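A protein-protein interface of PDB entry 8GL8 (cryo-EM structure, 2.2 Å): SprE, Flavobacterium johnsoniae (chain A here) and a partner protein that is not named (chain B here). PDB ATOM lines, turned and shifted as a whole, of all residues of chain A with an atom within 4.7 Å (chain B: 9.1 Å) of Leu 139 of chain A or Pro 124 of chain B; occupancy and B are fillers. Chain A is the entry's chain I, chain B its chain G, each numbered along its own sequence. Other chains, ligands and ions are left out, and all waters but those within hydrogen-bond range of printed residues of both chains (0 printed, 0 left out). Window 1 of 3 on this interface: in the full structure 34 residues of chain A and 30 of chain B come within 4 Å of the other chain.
Printed residues of chain B that touch a printed residue of chain A: Lys 123, Pro 124, Asp 127, Gln 128, Thr 174 and Asp 175.
Along chain B the printed residues that touch a printed residue of chain A span positions 123 to 175.
Of the 13 printed residues of chain A, 5 touch a printed residue of chain B.
Among the printed residues, Asp or Glu carboxylates within 4 Å of a Lys or Arg side-chain nitrogen of the other chain: Arg 162 of chain A with Asp 175 of chain B (3.9 Å).
The side-chain carboxylate (OD1) of Asp 175 of chain B lies within salt-bridge range of the guanidinium group (NH1) of Arg 162 of chain A.
Ala 138 of chain A touches none of the printed residues of chain B.
Leu 139 of chain A touches one residue of chain B.
Printed residues of chain B within 4 Å of Glu 140 of chain A: Asp 127 (3.6 Å).
Asp 41 of chain B touches none of the printed residues of chain A.
Ala 119 of chain B touches none of the printed residues of chain A.
Of the printed residues of chain A, Asp 127 of chain B touches Ile 136 and Glu 140.
Of the printed residues of chain A, Thr 174 of chain B touches Arg 162.
The nearest residue of chain B that does not touch Leu 139 of chain A is Asp 127 of chain B (6.1 Å).
The nearest printed residue of chain A that does not touch Asp 175 of chain B is Asn 143 of chain A (6.1 Å).
Among the printed residues, pairs that only touch across the chains: Asn 143 of chain A with Gln 128 of chain B, Glu 140 of chain A with Asp 127 of chain B, Arg 162 of chain A with Thr 174 of chain B, Ile 136 of chain A with Asp 127 of chain B, Leu 139 of chain A with Pro 124 of chain B and Ile 136 of chain A with Lys 123 of chain B.
The side-chain amide nitrogen (ND2) of Asn 143 of chain A sits close to the backbone carbonyl oxygen (O) of Leu 139 of chain A, 3.3 Å away.
O of Arg 162 of chain A lies within hydrogen-bond range of ND2 of Asn 166 of chain A, 3.1 Å away.
The backbone carbonyl oxygen of Leu 171 of chain B is in hydrogen-bond range of the side-chain hydroxyl of Thr 174 of chain B.
The side-chain amino group of Lys 123 of chain B lies within hydrogen-bond range of the backbone carbonyl oxygen of Ala 119 of chain B.
The backbone carbonyl oxygen (O) of Asp 127 of chain B lies within hydrogen-bond range of the side-chain hydroxyl (OG1) of Thr 131 of chain B (3.1 Å).
OE1 of Gln 128 of chain B lies within hydrogen-bond range of OG1 of Thr 174 of chain B, 3.4 Å away.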
ATOM      1  N   PHE A 135     -27.687 -20.315  10.957  1.00  0.00           N
ATOM      2  CA  PHE A 135     -28.197 -19.336  11.906  1.00  0.00           C
ATOM      3  C   PHE A 135     -27.294 -19.144  13.116  1.00  0.00           C
ATOM      4  O   PHE A 135     -27.240 -18.041  13.663  1.00  0.00           O
ATOM      5  CB  PHE A 135     -29.606 -19.731  12.341  1.00  0.00           C
ATOM      6  CG  PHE A 135     -30.581 -19.796  11.205  1.00  0.00           C
ATOM      7  CD1 PHE A 135     -30.759 -18.708  10.371  1.00  0.00           C
ATOM      8  CD2 PHE A 135     -31.303 -20.947  10.959  1.00  0.00           C
ATOM      9  CE1 PHE A 135     -31.647 -18.763   9.320  1.00  0.00           C
ATOM     10  CE2 PHE A 135     -32.194 -21.006   9.908  1.00  0.00           C
ATOM     11  CZ  PHE A 135     -32.365 -19.914   9.090  1.00  0.00           C
ATOM     12  N   ILE A 136     -26.585 -20.178  13.557  1.00  0.00           N
ATOM     13  CA  ILE A 136     -25.697 -20.026  14.709  1.00  0.00           C
ATOM     14  C   ILE A 136     -24.539 -19.085  14.373  1.00  0.00           C
ATOM     15  O   ILE A 136     -24.270 -18.162  15.156  1.00  0.00           O
ATOM     16  CB  ILE A 136     -25.201 -21.390  15.218  1.00  0.00           C
ATOM     17  CG1 ILE A 136     -26.388 -22.285  15.580  1.00  0.00           C
ATOM     18  CG2 ILE A 136     -24.272 -21.210  16.407  1.00  0.00           C
ATOM     19  CD1 ILE A 136     -26.862 -22.137  17.006  1.00  0.00           C
ATOM     20  N   PRO A 137     -23.817 -19.261  13.257  1.00  0.00           N
ATOM     21  CA  PRO A 137     -22.783 -18.266  12.916  1.00  0.00           C
ATOM     22  C   PRO A 137     -23.333 -16.875  12.637  1.00  0.00           C
ATOM     23  O   PRO A 137     -22.663 -15.880  12.947  1.00  0.00           O
ATOM     24  CB  PRO A 137     -22.106 -18.869  11.676  1.00  0.00           C
ATOM     25  CG  PRO A 137     -23.031 -19.898  11.176  1.00  0.00           C
ATOM     26  CD  PRO A 137     -23.750 -20.426  12.356  1.00  0.00           C
ATOM     27  N   ALA A 138     -24.532 -16.767  12.060  1.00  0.00           N
ATOM     28  CA  ALA A 138     -25.139 -15.456  11.852  1.00  0.00           C
ATOM     29  C   ALA A 138     -25.396 -14.760  13.181  1.00  0.00           C
ATOM     30  O   ALA A 138     -25.090 -13.571  13.352  1.00  0.00           O
ATOM     31  CB  ALA A 138     -26.436 -15.603  11.059  1.00  0.00           C
ATOM     32  N   LEU A 139     -25.952 -15.501  14.142  1.00  0.00           N
ATOM     33  CA  LEU A 139     -26.155 -14.965  15.480  1.00  0.00           C
ATOM     34  C   LEU A 139     -24.832 -14.580  16.117  1.00  0.00           C
ATOM     35  O   LEU A 139     -24.751 -13.577  16.831  1.00  0.00           O
ATOM     36  CB  LEU A 139     -26.889 -15.991  16.340  1.00  0.00           C
ATOM     37  CG  LEU A 139     -27.345 -15.575  17.738  1.00  0.00           C
ATOM     38  CD1 LEU A 139     -27.838 -14.146  17.745  1.00  0.00           C
ATOM     39  CD2 LEU A 139     -28.430 -16.509  18.219  1.00  0.00           C
ATOM     40  N   GLU A 140     -23.785 -15.370  15.877  1.00  0.00           N
ATOM     41  CA  GLU A 140     -22.472 -15.029  16.409  1.00  0.00           C
ATOM     42  C   GLU A 140     -21.978 -13.700  15.856  1.00  0.00           C
ATOM     43  O   GLU A 140     -21.438 -12.873  16.599  1.00  0.00           O
ATOM     44  CB  GLU A 140     -21.475 -16.143  16.098  1.00  0.00           C
ATOM     45  CG  GLU A 140     -20.266 -16.149  17.008  1.00  0.00           C
ATOM     46  CD  GLU A 140     -19.120 -16.955  16.445  1.00  0.00           C
ATOM     47  OE1 GLU A 140     -19.250 -17.466  15.314  1.00  0.00           O
ATOM     48  OE2 GLU A 140     -18.087 -17.080  17.136  1.00  0.00           O
ATOM     49  N   ALA A 141     -22.157 -13.475  14.554  1.00  0.00           N
ATOM     50  CA  ALA A 141     -21.739 -12.208  13.957  1.00  0.00           C
ATOM     51  C   ALA A 141     -22.523 -11.029  14.527  1.00  0.00           C
ATOM     52  O   ALA A 141     -21.942  -9.985  14.859  1.00  0.00           O
ATOM     53  CB  ALA A 141     -21.893 -12.272  12.439  1.00  0.00           C
ATOM     54  N   PHE A 142     -23.845 -11.176  14.652  1.00  0.00           N
ATOM     55  CA  PHE A 142     -24.651 -10.084  15.200  1.00  0.00           C
ATOM     56  C   PHE A 142     -24.291  -9.805  16.657  1.00  0.00           C
ATOM     57  O   PHE A 142     -24.195  -8.642  17.078  1.00  0.00           O
ATOM     58  CB  PHE A 142     -26.137 -10.402  15.057  1.00  0.00           C
ATOM     59  CG  PHE A 142     -26.589 -10.549  13.635  1.00  0.00           C
ATOM     60  CD1 PHE A 142     -26.233  -9.613  12.681  1.00  0.00           C
ATOM     61  CD2 PHE A 142     -27.369 -11.621  13.250  1.00  0.00           C
ATOM     62  CE1 PHE A 142     -26.644  -9.748  11.377  1.00  0.00           C
ATOM     63  CE2 PHE A 142     -27.780 -11.761  11.945  1.00  0.00           C
ATOM     64  CZ  PHE A 142     -27.418 -10.823  11.007  1.00  0.00           C
ATOM     65  N   ASN A 143     -24.075 -10.863  17.441  1.00  0.00           N
ATOM     66  CA  ASN A 143     -23.670 -10.691  18.829  1.00  0.00           C
ATOM     67  C   ASN A 143     -22.298 -10.046  18.932  1.00  0.00           C
ATOM     68  O   ASN A 143     -22.052  -9.263  19.852  1.00  0.00           O
ATOM     69  CB  ASN A 143     -23.679 -12.040  19.543  1.00  0.00           C
ATOM     70  CG  ASN A 143     -25.031 -12.381  20.119  1.00  0.00           C
ATOM     71  OD1 ASN A 143     -25.760 -11.506  20.578  1.00  0.00           O
ATOM     72  ND2 ASN A 143     -25.375 -13.660  20.098  1.00  0.00           N
ATOM     73  N   ARG A 162     -30.365 -10.053  15.198  1.00  0.00           N
ATOM     74  CA  ARG A 162     -30.186 -11.071  16.222  1.00  0.00           C
ATOM     75  C   ARG A 162     -31.521 -11.674  16.628  1.00  0.00           C
ATOM     76  O   ARG A 162     -31.630 -12.887  16.838  1.00  0.00           O
ATOM     77  CB  ARG A 162     -29.477 -10.463  17.431  1.00  0.00           C
ATOM     78  CG  ARG A 162     -29.677 -11.220  18.722  1.00  0.00           C
ATOM     79  CD  ARG A 162     -28.872 -10.608  19.846  1.00  0.00           C
ATOM     80  NE  ARG A 162     -29.625  -9.575  20.545  1.00  0.00           N
ATOM     81  CZ  ARG A 162     -29.189  -8.924  21.614  1.00  0.00           C
ATOM     82  NH1 ARG A 162     -28.000  -9.173  22.136  1.00  0.00           N
ATOM     83  NH2 ARG A 162     -29.966  -8.002  22.173  1.00  0.00           N
ATOM     84  N   THR A 165     -32.755 -13.970  13.867  1.00  0.00           N
ATOM     85  CA  THR A 165     -31.965 -15.193  13.924  1.00  0.00           C
ATOM     86  C   THR A 165     -32.432 -16.094  15.059  1.00  0.00           C
ATOM     87  O   THR A 165     -32.517 -17.316  14.897  1.00  0.00           O
ATOM     88  CB  THR A 165     -30.483 -14.860  14.081  1.00  0.00           C
ATOM     89  OG1 THR A 165     -30.094 -13.928  13.068  1.00  0.00           O
ATOM     90  CG2 THR A 165     -29.660 -16.107  13.932  1.00  0.00           C
ATOM     91  N   ASN A 166     -32.739 -15.505  16.217  1.00  0.00           N
ATOM     92  CA  ASN A 166     -33.287 -16.282  17.323  1.00  0.00           C
ATOM     93  C   ASN A 166     -34.631 -16.892  16.950  1.00  0.00           C
ATOM     94  O   ASN A 166     -34.932 -18.030  17.325  1.00  0.00           O
ATOM     95  CB  ASN A 166     -33.429 -15.401  18.562  1.00  0.00           C
ATOM     96  CG  ASN A 166     -32.189 -15.406  19.422  1.00  0.00           C
ATOM     97  OD1 ASN A 166     -31.757 -16.453  19.901  1.00  0.00           O
ATOM     98  ND2 ASN A 166     -31.608 -14.232  19.630  1.00  0.00           N
ATOM     99  N   LEU A 169     -34.113 -19.870  15.094  1.00  0.00           N
ATOM    100  CA  LEU A 169     -33.621 -20.929  15.964  1.00  0.00           C
ATOM    101  C   LEU A 169     -34.690 -21.470  16.906  1.00  0.00           C
ATOM    102  O   LEU A 169     -34.400 -22.379  17.688  1.00  0.00           O
ATOM    103  CB  LEU A 169     -32.425 -20.426  16.776  1.00  0.00           C
ATOM    104  CG  LEU A 169     -31.143 -20.160  15.988  1.00  0.00           C
ATOM    105  CD1 LEU A 169     -30.118 -19.459  16.854  1.00  0.00           C
ATOM    106  CD2 LEU A 169     -30.578 -21.450  15.429  1.00  0.00           C
ATOM    107  N   MET B  32     -19.000 -22.927  33.439  1.00  0.00           N
ATOM    108  CA  MET B  32     -20.012 -22.811  32.396  1.00  0.00           C
ATOM    109  C   MET B  32     -21.417 -22.991  32.957  1.00  0.00           C
ATOM    110  O   MET B  32     -22.356 -22.322  32.510  1.00  0.00           O
ATOM    111  CB  MET B  32     -19.739 -23.823  31.287  1.00  0.00           C
ATOM    112  CG  MET B  32     -20.283 -23.406  29.937  1.00  0.00           C
ATOM    113  SD  MET B  32     -19.775 -21.742  29.476  1.00  0.00           S
ATOM    114  CE  MET B  32     -20.965 -21.380  28.192  1.00  0.00           C
ATOM    115  N   LEU B  36     -24.306 -20.180  32.677  1.00  0.00           N
ATOM    116  CA  LEU B  36     -25.611 -20.496  32.105  1.00  0.00           C
ATOM    117  C   LEU B  36     -26.734 -20.269  33.107  1.00  0.00           C
ATOM    118  O   LEU B  36     -27.855 -19.928  32.714  1.00  0.00           O
ATOM    119  CB  LEU B  36     -25.626 -21.939  31.604  1.00  0.00           C
ATOM    120  CG  LEU B  36     -24.954 -22.190  30.254  1.00  0.00           C
ATOM    121  CD1 LEU B  36     -25.326 -23.557  29.720  1.00  0.00           C
ATOM    122  CD2 LEU B  36     -25.328 -21.107  29.262  1.00  0.00           C
ATOM    123  N   VAL B  39     -27.798 -16.380  33.208  1.00  0.00           N
ATOM    124  CA  VAL B  39     -28.253 -15.784  31.956  1.00  0.00           C
ATOM    125  C   VAL B  39     -29.761 -15.983  31.890  1.00  0.00           C
ATOM    126  O   VAL B  39     -30.241 -17.122  31.816  1.00  0.00           O
ATOM    127  CB  VAL B  39     -27.554 -16.394  30.734  1.00  0.00           C
ATOM    128  CG1 VAL B  39     -28.263 -15.981  29.458  1.00  0.00           C
ATOM    129  CG2 VAL B  39     -26.099 -15.966  30.689  1.00  0.00           C
ATOM    130  N   ASP B  41     -32.084 -15.110  29.586  1.00  0.00           N
ATOM    131  CA  ASP B  41     -32.665 -15.564  28.327  1.00  0.00           C
ATOM    132  C   ASP B  41     -32.494 -17.065  28.154  1.00  0.00           C
ATOM    133  O   ASP B  41     -33.386 -17.741  27.630  1.00  0.00           O
ATOM    134  CB  ASP B  41     -32.035 -14.808  27.158  1.00  0.00           C
ATOM    135  CG  ASP B  41     -32.812 -13.559  26.786  1.00  0.00           C
ATOM    136  OD1 ASP B  41     -33.803 -13.246  27.477  1.00  0.00           O
ATOM    137  OD2 ASP B  41     -32.432 -12.891  25.802  1.00  0.00           O
ATOM    138  N   TYR B  42     -31.356 -17.606  28.593  1.00  0.00           N
ATOM    139  CA  TYR B  42     -31.148 -19.048  28.525  1.00  0.00           C
ATOM    140  C   TYR B  42     -32.160 -19.794  29.384  1.00  0.00           C
ATOM    141  O   TYR B  42     -32.724 -20.807  28.955  1.00  0.00           O
ATOM    142  CB  TYR B  42     -29.723 -19.392  28.955  1.00  0.00           C
ATOM    143  CG  TYR B  42     -29.440 -20.873  28.969  1.00  0.00           C
ATOM    144  CD1 TYR B  42     -29.356 -21.591  27.786  1.00  0.00           C
ATOM    145  CD2 TYR B  42     -29.269 -21.555  30.162  1.00  0.00           C
ATOM    146  CE1 TYR B  42     -29.104 -22.942  27.792  1.00  0.00           C
ATOM    147  CE2 TYR B  42     -29.016 -22.907  30.177  1.00  0.00           C
ATOM    148  CZ  TYR B  42     -28.934 -23.595  28.989  1.00  0.00           C
ATOM    149  OH  TYR B  42     -28.681 -24.946  28.995  1.00  0.00           O
ATOM    150  N   ALA B  45     -35.574 -19.648  27.693  1.00  0.00           N
ATOM    151  CA  ALA B  45     -35.622 -20.560  26.558  1.00  0.00           C
ATOM    152  C   ALA B  45     -35.734 -22.007  27.018  1.00  0.00           C
ATOM    153  O   ALA B  45     -36.447 -22.810  26.406  1.00  0.00           O
ATOM    154  CB  ALA B  45     -34.389 -20.367  25.679  1.00  0.00           C
ATOM    155  N   GLN B 117     -32.661 -29.892  20.463  1.00  0.00           N
ATOM    156  CA  GLN B 117     -32.991 -28.504  20.757  1.00  0.00           C
ATOM    157  C   GLN B 117     -32.422 -28.060  22.096  1.00  0.00           C
ATOM    158  O   GLN B 117     -32.052 -26.892  22.252  1.00  0.00           O
ATOM    159  CB  GLN B 117     -34.505 -28.308  20.721  1.00  0.00           C
ATOM    160  CG  GLN B 117     -35.075 -28.294  19.316  1.00  0.00           C
ATOM    161  CD  GLN B 117     -36.580 -28.160  19.297  1.00  0.00           C
ATOM    162  OE1 GLN B 117     -37.156 -27.408  20.079  1.00  0.00           O
ATOM    163  NE2 GLN B 117     -37.227 -28.890  18.398  1.00  0.00           N
ATOM    164  N   LYS B 118     -32.353 -28.965  23.076  1.00  0.00           N
ATOM    165  CA  LYS B 118     -31.716 -28.629  24.345  1.00  0.00           C
ATOM    166  C   LYS B 118     -30.226 -28.377  24.166  1.00  0.00           C
ATOM    167  O   LYS B 118     -29.667 -27.465  24.784  1.00  0.00           O
ATOM    168  CB  LYS B 118     -31.949 -29.742  25.363  1.00  0.00           C
ATOM    169  CG  LYS B 118     -33.318 -29.721  26.006  1.00  0.00           C
ATOM    170  CD  LYS B 118     -33.223 -29.984  27.496  1.00  0.00           C
ATOM    171  CE  LYS B 118     -34.254 -31.001  27.942  1.00  0.00           C
ATOM    172  NZ  LYS B 118     -35.468 -30.348  28.499  1.00  0.00           N
ATOM    173  N   ALA B 119     -29.565 -29.180  23.328  1.00  0.00           N
ATOM    174  CA  ALA B 119     -28.129 -29.018  23.130  1.00  0.00           C
ATOM    175  C   ALA B 119     -27.800 -27.748  22.356  1.00  0.00           C
ATOM    176  O   ALA B 119     -26.706 -27.197  22.514  1.00  0.00           O
ATOM    177  CB  ALA B 119     -27.560 -30.238  22.409  1.00  0.00           C
ATOM    178  N   ALA B 120     -28.722 -27.271  21.524  1.00  0.00           N
ATOM    179  CA  ALA B 120     -28.481 -26.101  20.694  1.00  0.00           C
ATOM    180  C   ALA B 120     -28.802 -24.787  21.393  1.00  0.00           C
ATOM    181  O   ALA B 120     -28.551 -23.724  20.817  1.00  0.00           O
ATOM    182  CB  ALA B 120     -29.296 -26.199  19.402  1.00  0.00           C
ATOM    183  N   LEU B 121     -29.346 -24.830  22.610  1.00  0.00           N
ATOM    184  CA  LEU B 121     -29.730 -23.599  23.292  1.00  0.00           C
ATOM    185  C   LEU B 121     -28.514 -22.793  23.730  1.00  0.00           C
ATOM    186  O   LEU B 121     -28.519 -21.560  23.650  1.00  0.00           O
ATOM    187  CB  LEU B 121     -30.611 -23.921  24.496  1.00  0.00           C
ATOM    188  CG  LEU B 121     -32.118 -23.949  24.254  1.00  0.00           C
ATOM    189  CD1 LEU B 121     -32.856 -24.096  25.569  1.00  0.00           C
ATOM    190  CD2 LEU B 121     -32.561 -22.697  23.522  1.00  0.00           C
ATOM    191  N   ALA B 122     -27.469 -23.466  24.200  1.00  0.00           N
ATOM    192  CA  ALA B 122     -26.313 -22.797  24.776  1.00  0.00           C
ATOM    193  C   ALA B 122     -25.239 -22.453  23.754  1.00  0.00           C
ATOM    194  O   ALA B 122     -24.236 -21.837  24.124  1.00  0.00           O
ATOM    195  CB  ALA B 122     -25.706 -23.663  25.882  1.00  0.00           C
ATOM    196  N   LYS B 123     -25.415 -22.834  22.489  1.00  0.00           N
ATOM    197  CA  LYS B 123     -24.374 -22.587  21.493  1.00  0.00           C
ATOM    198  C   LYS B 123     -24.075 -21.105  21.295  1.00  0.00           C
ATOM    199  O   LYS B 123     -22.887 -20.738  21.286  1.00  0.00           O
ATOM    200  CB  LYS B 123     -24.752 -23.271  20.176  1.00  0.00           C
ATOM    201  CG  LYS B 123     -24.403 -24.744  20.118  1.00  0.00           C
ATOM    202  CD  LYS B 123     -24.925 -25.377  18.844  1.00  0.00           C
ATOM    203  CE  LYS B 123     -24.559 -26.847  18.764  1.00  0.00           C
ATOM    204  NZ  LYS B 123     -24.229 -27.411  20.097  1.00  0.00           N
ATOM    205  N   PRO B 124     -25.060 -20.211  21.111  1.00  0.00           N
ATOM    206  CA  PRO B 124     -24.717 -18.778  21.061  1.00  0.00           C
ATOM    207  C   PRO B 124     -24.073 -18.271  22.338  1.00  0.00           C
ATOM    208  O   PRO B 124     -23.157 -17.437  22.286  1.00  0.00           O
ATOM    209  CB  PRO B 124     -26.071 -18.102  20.796  1.00  0.00           C
ATOM    210  CG  PRO B 124     -27.094 -19.122  21.115  1.00  0.00           C
ATOM    211  CD  PRO B 124     -26.483 -20.432  20.804  1.00  0.00           C
ATOM    212  N   ILE B 125     -24.524 -18.763  23.493  1.00  0.00           N
ATOM    213  CA  ILE B 125     -23.900 -18.375  24.752  1.00  0.00           C
ATOM    214  C   ILE B 125     -22.467 -18.877  24.806  1.00  0.00           C
ATOM    215  O   ILE B 125     -21.576 -18.189  25.312  1.00  0.00           O
ATOM    216  CB  ILE B 125     -24.723 -18.887  25.947  1.00  0.00           C
ATOM    217  CG1 ILE B 125     -26.214 -18.647  25.710  1.00  0.00           C
ATOM    218  CG2 ILE B 125     -24.260 -18.219  27.229  1.00  0.00           C
ATOM    219  CD1 ILE B 125     -26.684 -17.277  26.119  1.00  0.00           C
ATOM    220  N   GLN B 126     -22.219 -20.083  24.291  1.00  0.00           N
ATOM    221  CA  GLN B 126     -20.855 -20.598  24.242  1.00  0.00           C
ATOM    222  C   GLN B 126     -19.977 -19.745  23.336  1.00  0.00           C
ATOM    223  O   GLN B 126     -18.814 -19.488  23.659  1.00  0.00           O
ATOM    224  CB  GLN B 126     -20.858 -22.050  23.772  1.00  0.00           C
ATOM    225  CG  GLN B 126     -21.341 -23.040  24.808  1.00  0.00           C
ATOM    226  CD  GLN B 126     -21.240 -24.467  24.325  1.00  0.00           C
ATOM    227  OE1 GLN B 126     -20.148 -25.018  24.213  1.00  0.00           O
ATOM    228  NE2 GLN B 126     -22.381 -25.074  24.026  1.00  0.00           N
ATOM    229  N   ASP B 127     -20.513 -19.304  22.196  1.00  0.00           N
ATOM    230  CA  ASP B 127     -19.764 -18.415  21.313  1.00  0.00           C
ATOM    231  C   ASP B 127     -19.394 -17.118  22.023  1.00  0.00           C
ATOM    232  O   ASP B 127     -18.236 -16.674  21.982  1.00  0.00           O
ATOM    233  CB  ASP B 127     -20.587 -18.111  20.062  1.00  0.00           C
ATOM    234  CG  ASP B 127     -20.733 -19.307  19.155  1.00  0.00           C
ATOM    235  OD1 ASP B 127     -19.889 -20.220  19.233  1.00  0.00           O
ATOM    236  OD2 ASP B 127     -21.696 -19.338  18.361  1.00  0.00           O
ATOM    237  N   GLN B 128     -20.374 -16.493  22.679  1.00  0.00           N
ATOM    238  CA  GLN B 128     -20.114 -15.243  23.384  1.00  0.00           C
ATOM    239  C   GLN B 128     -19.110 -15.441  24.509  1.00  0.00           C
ATOM    240  O   GLN B 128     -18.224 -14.603  24.716  1.00  0.00           O
ATOM    241  CB  GLN B 128     -21.417 -14.670  23.930  1.00  0.00           C
ATOM    242  CG  GLN B 128     -22.390 -14.212  22.869  1.00  0.00           C
ATOM    243  CD  GLN B 128     -23.668 -13.671  23.463  1.00  0.00           C
ATOM    244  OE1 GLN B 128     -23.746 -12.502  23.835  1.00  0.00           O
ATOM    245  NE2 GLN B 128     -24.679 -14.523  23.562  1.00  0.00           N
ATOM    246  N   VAL B 129     -19.233 -16.545  25.248  1.00  0.00           N
ATOM    247  CA  VAL B 129     -18.310 -16.825  26.342  1.00  0.00           C
ATOM    248  C   VAL B 129     -16.902 -17.039  25.811  1.00  0.00           C
ATOM    249  O   VAL B 129     -15.929 -16.563  26.400  1.00  0.00           O
ATOM    250  CB  VAL B 129     -18.804 -18.034  27.156  1.00  0.00           C
ATOM    251  CG1 VAL B 129     -17.681 -18.602  28.007  1.00  0.00           C
ATOM    252  CG2 VAL B 129     -19.976 -17.637  28.027  1.00  0.00           C
ATOM    253  N   PHE B 130     -16.766 -17.760  24.698  1.00  0.00           N
ATOM    254  CA  PHE B 130     -15.448 -17.981  24.114  1.00  0.00           C
ATOM    255  C   PHE B 130     -14.806 -16.664  23.701  1.00  0.00           C
ATOM    256  O   PHE B 130     -13.627 -16.419  23.984  1.00  0.00           O
ATOM    257  CB  PHE B 130     -15.559 -18.928  22.920  1.00  0.00           C
ATOM    258  CG  PHE B 130     -14.240 -19.279  22.302  1.00  0.00           C
ATOM    259  CD1 PHE B 130     -13.470 -20.303  22.822  1.00  0.00           C
ATOM    260  CD2 PHE B 130     -13.764 -18.581  21.206  1.00  0.00           C
ATOM    261  CE1 PHE B 130     -12.255 -20.626  22.260  1.00  0.00           C
ATOM    262  CE2 PHE B 130     -12.552 -18.899  20.642  1.00  0.00           C
ATOM    263  CZ  PHE B 130     -11.796 -19.923  21.168  1.00  0.00           C
ATOM    264  N   THR B 131     -15.574 -15.795  23.038  1.00  0.00           N
ATOM    265  CA  THR B 131     -15.025 -14.504  22.628  1.00  0.00           C
ATOM    266  C   THR B 131     -14.628 -13.659  23.835  1.00  0.00           C
ATOM    267  O   THR B 131     -13.545 -13.055  23.856  1.00  0.00           O
ATOM    268  CB  THR B 131     -16.035 -13.759  21.758  1.00  0.00           C
ATOM    269  OG1 THR B 131     -16.371 -14.563  20.622  1.00  0.00           O
ATOM    270  CG2 THR B 131     -15.451 -12.447  21.278  1.00  0.00           C
ATOM    271  N   ALA B 132     -15.488 -13.616  24.856  1.00  0.00           N
ATOM    272  CA  ALA B 132     -15.180 -12.844  26.053  1.00  0.00           C
ATOM    273  C   ALA B 132     -13.955 -13.394  26.766  1.00  0.00           C
ATOM    274  O   ALA B 132     -13.150 -12.630  27.303  1.00  0.00           O
ATOM    275  CB  ALA B 132     -16.385 -12.830  26.992  1.00  0.00           C
ATOM    276  N   LEU B 171     -21.526 -10.399  29.172  1.00  0.00           N
ATOM    277  CA  LEU B 171     -22.694 -10.922  28.470  1.00  0.00           C
ATOM    278  C   LEU B 171     -23.914 -10.041  28.699  1.00  0.00           C
ATOM    279  O   LEU B 171     -24.673  -9.763  27.762  1.00  0.00           O
ATOM    280  CB  LEU B 171     -22.975 -12.354  28.921  1.00  0.00           C
ATOM    281  CG  LEU B 171     -22.574 -13.479  27.964  1.00  0.00           C
ATOM    282  CD1 LEU B 171     -21.085 -13.441  27.683  1.00  0.00           C
ATOM    283  CD2 LEU B 171     -22.972 -14.823  28.535  1.00  0.00           C
ATOM    284  N   THR B 174     -23.508  -6.762  26.619  1.00  0.00           N
ATOM    285  CA  THR B 174     -23.881  -6.878  25.210  1.00  0.00           C
ATOM    286  C   THR B 174     -25.368  -7.161  25.039  1.00  0.00           C
ATOM    287  O   THR B 174     -25.952  -6.778  24.021  1.00  0.00           O
ATOM    288  CB  THR B 174     -23.072  -7.962  24.494  1.00  0.00           C
ATOM    289  OG1 THR B 174     -23.765  -9.212  24.562  1.00  0.00           O
ATOM    290  CG2 THR B 174     -21.698  -8.099  25.084  1.00  0.00           C
ATOM    291  N   ASP B 175     -25.995  -7.833  26.006  1.00  0.00           N
ATOM    292  CA  ASP B 175     -27.428  -8.083  25.899  1.00  0.00           C
ATOM    293  C   ASP B 175     -28.227  -6.789  26.000  1.00  0.00           C
ATOM    294  O   ASP B 175     -29.196  -6.593  25.256  1.00  0.00           O
ATOM    295  CB  ASP B 175     -27.875  -9.070  26.973  1.00  0.00           C
ATOM    296  CG  ASP B 175     -29.132  -9.816  26.587  1.00  0.00           C
ATOM    297  OD1 ASP B 175     -29.105 -10.539  25.569  1.00  0.00           O
ATOM    298  OD2 ASP B 175     -30.151  -9.678  27.295  1.00  0.00           O
